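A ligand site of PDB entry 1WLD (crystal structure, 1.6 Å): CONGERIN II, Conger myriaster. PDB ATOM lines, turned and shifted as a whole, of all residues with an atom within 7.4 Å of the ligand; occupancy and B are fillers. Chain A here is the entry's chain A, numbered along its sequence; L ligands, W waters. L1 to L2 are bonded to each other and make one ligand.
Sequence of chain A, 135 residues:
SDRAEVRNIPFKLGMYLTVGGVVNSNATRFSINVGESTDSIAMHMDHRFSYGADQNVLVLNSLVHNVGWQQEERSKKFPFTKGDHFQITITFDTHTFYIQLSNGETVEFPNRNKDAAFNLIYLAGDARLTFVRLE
The side-chain carboxylate (OE2) of Glu 72 sits at hydrogen-bond distance from an oxygen (O3) of LIG L1, 2.4 Å away.
NE2 of His 44 lies within hydrogen-bond range of O3 of LG2 L2 (2.7 Å).
An oxygen (O1) of LG2 L2 lies within hydrogen-bond range of the side-chain hydroxyl of Tyr 51.
The side-chain amide nitrogen of Asn 61 lies within hydrogen-bond range of an oxygen (O5) of LG2 L2, at 2.8 Å.
The guanidinium group (NH2) of Arg 48 is in hydrogen-bond range of an oxygen (O4) of LG2 L2 (2.9 Å).
The guanidinium group (NH2) of Arg 29 lies within hydrogen-bond range of an oxygen (O2) of LG2 L2, 2.9 Å away.
NH2 of Arg 74 sits at hydrogen-bond distance from O2 of LIG L1 (3.4 Å).
The side-chain carboxylate (OE1) of Glu 72 lies within salt-bridge range of the guanidinium group (NH2) of Arg 74.
The backbone NH (N) of His 44 sits at hydrogen-bond distance from the backbone carbonyl oxygen (O) of Asn 61 (2.9 Å).
The side-chain amide nitrogen of Asn 61 is in hydrogen-bond range of the backbone carbonyl oxygen of Gln 70 (2.8 Å).
OD1 of Asn 61 lies close to O of Gln 71 (3.2 Å).
The side-chain carboxylate of Asp 46 is in salt-bridge range of the guanidinium group of Arg 48 (2.8 Å).
NH1 of Arg 48 is in salt-bridge range of OD2 of Asp 54 (2.6 Å).
OD2 of Asp 46 lies within salt-bridge range of NH2 of Arg 29.
The backbone NH (N) of Asp 46 lies within hydrogen-bond range of the backbone carbonyl oxygen (O) of Val 59 (2.8 Å).
Residues that only touch the ligand: Asp 46 and Trp 69.
The nearest printed residue that does not touch the ligand is Val 59 (4.3 Å).
Water W4 bridges an oxygen (O5) of LG2 L2 (3.0 Å) and the side-chain carboxylate of Glu 72 (3.2 Å).
Water W1 lies within hydrogen-bond range of NH1 of Arg 29 (2.8 Å) and O2 of LG2 L2 (3.1 Å).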
ATOM      1  N   ARG A  29      11.910 -13.867  25.216  1.00  0.00           N
ATOM      2  CA  ARG A  29      11.605 -12.460  25.310  1.00  0.00           C
ATOM      3  C   ARG A  29      11.051 -12.126  26.704  1.00  0.00           C
ATOM      4  O   ARG A  29      10.448 -13.013  27.330  1.00  0.00           O
ATOM      5  CB  ARG A  29      10.569 -12.062  24.210  1.00  0.00           C
ATOM      6  CG  ARG A  29       9.329 -12.944  24.315  1.00  0.00           C
ATOM      7  CD  ARG A  29       8.380 -12.916  23.138  1.00  0.00           C
ATOM      8  NE  ARG A  29       7.676 -11.656  23.061  1.00  0.00           N
ATOM      9  CZ  ARG A  29       6.380 -11.410  23.066  1.00  0.00           C
ATOM     10  NH1 ARG A  29       5.394 -12.281  23.156  1.00  0.00           N
ATOM     11  NH2 ARG A  29       6.004 -10.134  22.977  1.00  0.00           N
ATOM     12  N   SER A  31       9.246  -8.385  28.745  1.00  0.00           N
ATOM     13  CA  SER A  31       8.949  -6.949  28.517  1.00  0.00           C
ATOM     14  C   SER A  31       8.865  -6.192  29.836  1.00  0.00           C
ATOM     15  O   SER A  31       8.567  -6.801  30.868  1.00  0.00           O
ATOM     16  CB  SER A  31       7.620  -6.829  27.745  1.00  0.00           C
ATOM     17  OG  SER A  31       6.557  -7.398  28.510  1.00  0.00           O
ATOM     18  N   ASN A  33       6.659  -2.887  31.271  1.00  0.00           N
ATOM     19  CA  ASN A  33       5.405  -2.279  30.825  1.00  0.00           C
ATOM     20  C   ASN A  33       4.946  -1.187  31.790  1.00  0.00           C
ATOM     21  O   ASN A  33       4.991  -1.431  32.996  1.00  0.00           O
ATOM     22  CB  ASN A  33       4.273  -3.335  30.797  1.00  0.00           C
ATOM     23  CG  ASN A  33       4.622  -4.478  29.860  1.00  0.00           C
ATOM     24  OD1 ASN A  33       4.335  -4.380  28.665  1.00  0.00           O
ATOM     25  ND2 ASN A  33       5.279  -5.532  30.368  1.00  0.00           N
ATOM     26  N   HIS A  44       5.205  -0.253  26.333  1.00  0.00           N
ATOM     27  CA  HIS A  44       5.665  -1.622  26.360  1.00  0.00           C
ATOM     28  C   HIS A  44       7.022  -1.717  25.693  1.00  0.00           C
ATOM     29  O   HIS A  44       7.135  -1.285  24.537  1.00  0.00           O
ATOM     30  CB  HIS A  44       4.670  -2.506  25.613  1.00  0.00           C
ATOM     31  CG  HIS A  44       5.044  -3.879  25.218  1.00  0.00           C
ATOM     32  ND1 HIS A  44       5.014  -4.948  26.089  1.00  0.00           N
ATOM     33  CD2 HIS A  44       5.415  -4.387  24.005  1.00  0.00           C
ATOM     34  CE1 HIS A  44       5.337  -6.051  25.425  1.00  0.00           C
ATOM     35  NE2 HIS A  44       5.604  -5.744  24.177  1.00  0.00           N
ATOM     36  N   MET A  45       8.011  -2.253  26.391  1.00  0.00           N
ATOM     37  CA  MET A  45       9.332  -2.427  25.774  1.00  0.00           C
ATOM     38  C   MET A  45       9.697  -3.904  25.849  1.00  0.00           C
ATOM     39  O   MET A  45       9.939  -4.424  26.942  1.00  0.00           O
ATOM     40  CB  MET A  45      10.416  -1.598  26.472  1.00  0.00           C
ATOM     41  CG  MET A  45      11.767  -1.842  25.765  1.00  0.00           C
ATOM     42  SD  MET A  45      13.086  -0.677  26.189  1.00  0.00           S
ATOM     43  CE  MET A  45      12.918  -0.871  27.990  1.00  0.00           C
ATOM     44  N   ASP A  46       9.721  -4.571  24.697  1.00  0.00           N
ATOM     45  CA  ASP A  46       9.921  -6.002  24.643  1.00  0.00           C
ATOM     46  C   ASP A  46      11.378  -6.277  24.259  1.00  0.00           C
ATOM     47  O   ASP A  46      11.891  -5.651  23.328  1.00  0.00           O
ATOM     48  CB  ASP A  46       8.935  -6.627  23.628  1.00  0.00           C
ATOM     49  CG  ASP A  46       8.767  -8.113  23.780  1.00  0.00           C
ATOM     50  OD1 ASP A  46       9.076  -8.658  24.873  1.00  0.00           O
ATOM     51  OD2 ASP A  46       8.372  -8.770  22.787  1.00  0.00           O
ATOM     52  N   ARG A  48      13.623  -8.971  22.773  1.00  0.00           N
ATOM     53  CA  ARG A  48      13.436 -10.196  22.020  1.00  0.00           C
ATOM     54  C   ARG A  48      14.768 -10.883  21.713  1.00  0.00           C
ATOM     55  O   ARG A  48      15.536 -10.353  20.924  1.00  0.00           O
ATOM     56  CB  ARG A  48      12.663  -9.886  20.728  1.00  0.00           C
ATOM     57  CG  ARG A  48      11.251  -9.358  21.053  1.00  0.00           C
ATOM     58  CD  ARG A  48      10.502  -8.982  19.769  1.00  0.00           C
ATOM     59  NE  ARG A  48       9.137  -8.539  20.139  1.00  0.00           N
ATOM     60  CZ  ARG A  48       8.145  -8.309  19.302  1.00  0.00           C
ATOM     61  NH1 ARG A  48       8.405  -8.498  17.995  1.00  0.00           N
ATOM     62  NH2 ARG A  48       6.948  -7.925  19.708  1.00  0.00           N
ATOM     63  N   TYR A  51      12.235 -14.363  18.775  1.00  0.00           N
ATOM     64  CA  TYR A  51      10.769 -14.266  18.669  1.00  0.00           C
ATOM     65  C   TYR A  51      10.394 -14.073  17.198  1.00  0.00           C
ATOM     66  O   TYR A  51      10.583 -13.003  16.620  1.00  0.00           O
ATOM     67  CB  TYR A  51      10.227 -13.125  19.511  1.00  0.00           C
ATOM     68  CG  TYR A  51       8.727 -12.936  19.485  1.00  0.00           C
ATOM     69  CD1 TYR A  51       7.897 -13.909  19.995  1.00  0.00           C
ATOM     70  CD2 TYR A  51       8.149 -11.811  18.915  1.00  0.00           C
ATOM     71  CE1 TYR A  51       6.516 -13.777  19.988  1.00  0.00           C
ATOM     72  CE2 TYR A  51       6.767 -11.656  18.879  1.00  0.00           C
ATOM     73  CZ  TYR A  51       5.968 -12.639  19.434  1.00  0.00           C
ATOM     74  OH  TYR A  51       4.594 -12.505  19.387  1.00  0.00           O
ATOM     75  N   ALA A  53      10.852 -13.697  13.659  1.00  0.00           N
ATOM     76  CA  ALA A  53      11.988 -13.225  12.892  1.00  0.00           C
ATOM     77  C   ALA A  53      12.887 -12.250  13.647  1.00  0.00           C
ATOM     78  O   ALA A  53      13.927 -11.823  13.145  1.00  0.00           O
ATOM     79  CB  ALA A  53      11.492 -12.473  11.644  1.00  0.00           C
ATOM     80  N   ASP A  54      12.466 -11.843  14.845  1.00  0.00           N
ATOM     81  CA  ASP A  54      13.220 -10.916  15.663  1.00  0.00           C
ATOM     82  C   ASP A  54      14.243 -11.629  16.540  1.00  0.00           C
ATOM     83  O   ASP A  54      13.889 -12.444  17.388  1.00  0.00           O
ATOM     84  CB  ASP A  54      12.263 -10.137  16.582  1.00  0.00           C
ATOM     85  CG  ASP A  54      11.354  -9.220  15.788  1.00  0.00           C
ATOM     86  OD1 ASP A  54      11.854  -8.647  14.801  1.00  0.00           O
ATOM     87  OD2 ASP A  54      10.175  -9.029  16.137  1.00  0.00           O
ATOM     88  N   VAL A  59      11.569  -4.044  20.866  1.00  0.00           N
ATOM     89  CA  VAL A  59      10.348  -3.624  20.161  1.00  0.00           C
ATOM     90  C   VAL A  59       9.462  -2.856  21.143  1.00  0.00           C
ATOM     91  O   VAL A  59       9.177  -3.419  22.221  1.00  0.00           O
ATOM     92  CB  VAL A  59       9.575  -4.827  19.589  1.00  0.00           C
ATOM     93  CG1 VAL A  59       8.312  -4.348  18.900  1.00  0.00           C
ATOM     94  CG2 VAL A  59      10.459  -5.582  18.577  1.00  0.00           C
ATOM     95  N   LEU A  60       9.144  -1.623  20.829  1.00  0.00           N
ATOM     96  CA  LEU A  60       8.338  -0.791  21.728  1.00  0.00           C
ATOM     97  C   LEU A  60       6.969  -0.484  21.132  1.00  0.00           C
ATOM     98  O   LEU A  60       6.804  -0.285  19.903  1.00  0.00           O
ATOM     99  CB  LEU A  60       9.062   0.531  22.002  1.00  0.00           C
ATOM    100  CG  LEU A  60      10.388   0.383  22.751  1.00  0.00           C
ATOM    101  CD1 LEU A  60      11.549   0.193  21.769  1.00  0.00           C
ATOM    102  CD2 LEU A  60      10.635   1.617  23.597  1.00  0.00           C
ATOM    103  N   ASN A  61       5.942  -0.402  21.980  1.00  0.00           N
ATOM    104  CA  ASN A  61       4.588  -0.134  21.436  1.00  0.00           C
ATOM    105  C   ASN A  61       3.673   0.256  22.586  1.00  0.00           C
ATOM    106  O   ASN A  61       4.109   0.276  23.723  1.00  0.00           O
ATOM    107  CB  ASN A  61       4.066  -1.362  20.694  1.00  0.00           C
ATOM    108  CG  ASN A  61       3.021  -1.027  19.630  1.00  0.00           C
ATOM    109  OD1 ASN A  61       2.554   0.118  19.599  1.00  0.00           O
ATOM    110  ND2 ASN A  61       2.674  -1.983  18.761  1.00  0.00           N
ATOM    111  N   SER A  62       2.457   0.651  22.247  1.00  0.00           N
ATOM    112  CA  SER A  62       1.401   0.891  23.230  1.00  0.00           C
ATOM    113  C   SER A  62       0.248  -0.066  22.960  1.00  0.00           C
ATOM    114  O   SER A  62       0.013  -0.487  21.826  1.00  0.00           O
ATOM    115  CB  SER A  62       0.919   2.346  23.204  1.00  0.00           C
ATOM    116  OG  SER A  62       0.578   2.695  21.860  1.00  0.00           O
ATOM    117  N   TRP A  69      -2.675  -3.475  19.783  1.00  0.00           N
ATOM    118  CA  TRP A  69      -1.366  -2.871  19.645  1.00  0.00           C
ATOM    119  C   TRP A  69      -1.383  -1.813  18.550  1.00  0.00           C
ATOM    120  O   TRP A  69      -2.064  -1.966  17.514  1.00  0.00           O
ATOM    121  CB  TRP A  69      -0.320  -3.942  19.356  1.00  0.00           C
ATOM    122  CG  TRP A  69      -0.140  -4.858  20.538  1.00  0.00           C
ATOM    123  CD1 TRP A  69      -0.633  -6.105  20.716  1.00  0.00           C
ATOM    124  CD2 TRP A  69       0.591  -4.536  21.746  1.00  0.00           C
ATOM    125  NE1 TRP A  69      -0.264  -6.612  21.935  1.00  0.00           N
ATOM    126  CE2 TRP A  69       0.483  -5.657  22.580  1.00  0.00           C
ATOM    127  CE3 TRP A  69       1.321  -3.445  22.182  1.00  0.00           C
ATOM    128  CZ2 TRP A  69       1.098  -5.717  23.847  1.00  0.00           C
ATOM    129  CZ3 TRP A  69       1.911  -3.479  23.446  1.00  0.00           C
ATOM    130  CH2 TRP A  69       1.795  -4.616  24.247  1.00  0.00           C
ATOM    131  N   GLN A  70      -0.701  -0.719  18.836  1.00  0.00           N
ATOM    132  CA  GLN A  70      -0.577   0.398  17.902  1.00  0.00           C
ATOM    133  C   GLN A  70       0.666   0.234  17.018  1.00  0.00           C
ATOM    134  O   GLN A  70       1.028  -0.899  16.704  1.00  0.00           O
ATOM    135  CB  GLN A  70      -0.629   1.699  18.698  1.00  0.00           C
ATOM    136  CG  GLN A  70      -1.931   1.806  19.548  1.00  0.00           C
ATOM    137  CD  GLN A  70      -3.161   1.629  18.666  1.00  0.00           C
ATOM    138  OE1 GLN A  70      -3.330   2.416  17.743  1.00  0.00           O
ATOM    139  NE2 GLN A  70      -4.012   0.645  18.906  1.00  0.00           N
ATOM    140  N   GLN A  71       1.284   1.349  16.661  1.00  0.00           N
ATOM    141  CA  GLN A  71       2.406   1.297  15.720  1.00  0.00           C
ATOM    142  C   GLN A  71       3.700   0.960  16.474  1.00  0.00           C
ATOM    143  O   GLN A  71       4.134   1.735  17.327  1.00  0.00           O
ATOM    144  CB  GLN A  71       2.542   2.618  14.984  1.00  0.00           C
ATOM    145  CG  GLN A  71       3.832   2.784  14.197  1.00  0.00           C
ATOM    146  CD  GLN A  71       3.878   1.859  13.004  1.00  0.00           C
ATOM    147  OE1 GLN A  71       3.035   2.005  12.098  1.00  0.00           O
ATOM    148  NE2 GLN A  71       4.839   0.935  12.983  1.00  0.00           N
ATOM    149  N   GLU A  72       4.316  -0.157  16.085  1.00  0.00           N
ATOM    150  CA  GLU A  72       5.583  -0.527  16.709  1.00  0.00           C
ATOM    151  C   GLU A  72       6.744   0.387  16.317  1.00  0.00           C
ATOM    152  O   GLU A  72       6.855   0.828  15.181  1.00  0.00           O
ATOM    153  CB  GLU A  72       6.044  -1.923  16.257  1.00  0.00           C
ATOM    154  CG  GLU A  72       5.225  -3.055  16.799  1.00  0.00           C
ATOM    155  CD  GLU A  72       5.781  -4.404  16.397  1.00  0.00           C
ATOM    156  OE1 GLU A  72       6.715  -4.529  15.551  1.00  0.00           O
ATOM    157  OE2 GLU A  72       5.212  -5.352  16.934  1.00  0.00           O
ATOM    158  N   GLU A  73       7.661   0.552  17.254  1.00  0.00           N
ATOM    159  CA  GLU A  73       8.966   1.174  17.045  1.00  0.00           C
ATOM    160  C   GLU A  73      10.011   0.134  17.419  1.00  0.00           C
ATOM    161  O   GLU A  73       9.790  -0.731  18.278  1.00  0.00           O
ATOM    162  CB  GLU A  73       9.110   2.451  17.874  1.00  0.00           C
ATOM    163  CG  GLU A  73       8.134   3.532  17.454  1.00  0.00           C
ATOM    164  CD  GLU A  73       8.412   4.917  17.937  1.00  0.00           C
ATOM    165  OE1 GLU A  73       7.699   5.845  17.473  1.00  0.00           O
ATOM    166  OE2 GLU A  73       9.294   5.212  18.763  1.00  0.00           O
ATOM    167  N   ARG A  74      11.121   0.095  16.691  1.00  0.00           N
ATOM    168  CA  ARG A  74      12.162  -0.876  16.997  1.00  0.00           C
ATOM    169  C   ARG A  74      13.502  -0.203  17.265  1.00  0.00           C
ATOM    170  O   ARG A  74      13.781   0.899  16.806  1.00  0.00           O
ATOM    171  CB  ARG A  74      12.277  -1.857  15.813  1.00  0.00           C
ATOM    172  CG  ARG A  74      11.040  -2.736  15.776  1.00  0.00           C
ATOM    173  CD  ARG A  74      10.975  -3.713  14.622  1.00  0.00           C
ATOM    174  NE  ARG A  74       9.770  -4.563  14.867  1.00  0.00           N
ATOM    175  CZ  ARG A  74       9.912  -5.884  14.870  1.00  0.00           C
ATOM    176  NH1 ARG A  74      11.127  -6.339  14.635  1.00  0.00           N
ATOM    177  NH2 ARG A  74       8.861  -6.662  15.096  1.00  0.00           N
HETATM  178  C1  LIG L   1       4.853  -8.210  14.605  1.00  0.00           C
HETATM  179  C2  LIG L   1       5.088  -8.568  16.072  1.00  0.00           C
HETATM  180  C3  LIG L   1       3.759  -8.619  16.818  1.00  0.00           C
HETATM  181  C4  LIG L   1       2.838  -9.590  16.069  1.00  0.00           C
HETATM  182  C5  LIG L   1       1.478  -9.721  16.642  1.00  0.00           C
HETATM  183  C6  LIG L   1       3.908  -9.221  14.013  1.00  0.00           C
HETATM  184  O1  LIG L   1       3.621  -8.479  12.619  1.00  0.00           O
HETATM  185  O2  LIG L   1       6.110  -8.284  13.941  1.00  0.00           O
HETATM  186  O3  LIG L   1       5.965  -7.644  16.647  1.00  0.00           O
HETATM  187  O4  LIG L   1       3.986  -9.163  18.090  1.00  0.00           O
HETATM  188  O5  LIG L   1       2.669  -9.090  14.703  1.00  0.00           O
HETATM  189  O6  LIG L   1       0.828  -8.474  16.910  1.00  0.00           O
HETATM  190  C1  LG2 L   2       3.404  -8.445  19.165  1.00  0.00           C
HETATM  191  C2  LG2 L   2       3.617  -9.302  20.417  1.00  0.00           C
HETATM  192  C3  LG2 L   2       3.124  -8.603  21.497  1.00  0.00           C
HETATM  193  C4  LG2 L   2       3.830  -7.203  21.742  1.00  0.00           C
HETATM  194  C5  LG2 L   2       3.646  -6.458  20.418  1.00  0.00           C
HETATM  195  C6  LG2 L   2       4.396  -5.141  20.351  1.00  0.00           C
HETATM  196  O1  LG2 L   2       2.867 -10.498  20.277  1.00  0.00           O
HETATM  197  O2  LG2 L   2       3.213  -9.336  22.785  1.00  0.00           O
HETATM  198  O3  LG2 L   2       5.204  -7.423  22.048  1.00  0.00           O
HETATM  199  O4  LG2 L   2       4.155  -7.240  19.316  1.00  0.00           O
HETATM  200  O5  LG2 L   2       3.979  -4.462  19.153  1.00  0.00           O
HETATM  201  O   HOH W   1       2.606 -12.327  23.008  1.00  0.00           O
HETATM  202  O   HOH W   2       0.141 -11.098  20.202  1.00  0.00           O
HETATM  203  O   HOH W   3       2.238  -6.029  12.720  1.00  0.00           O
HETATM  204  O   HOH W   4       2.042  -5.221  16.942  1.00  0.00           O
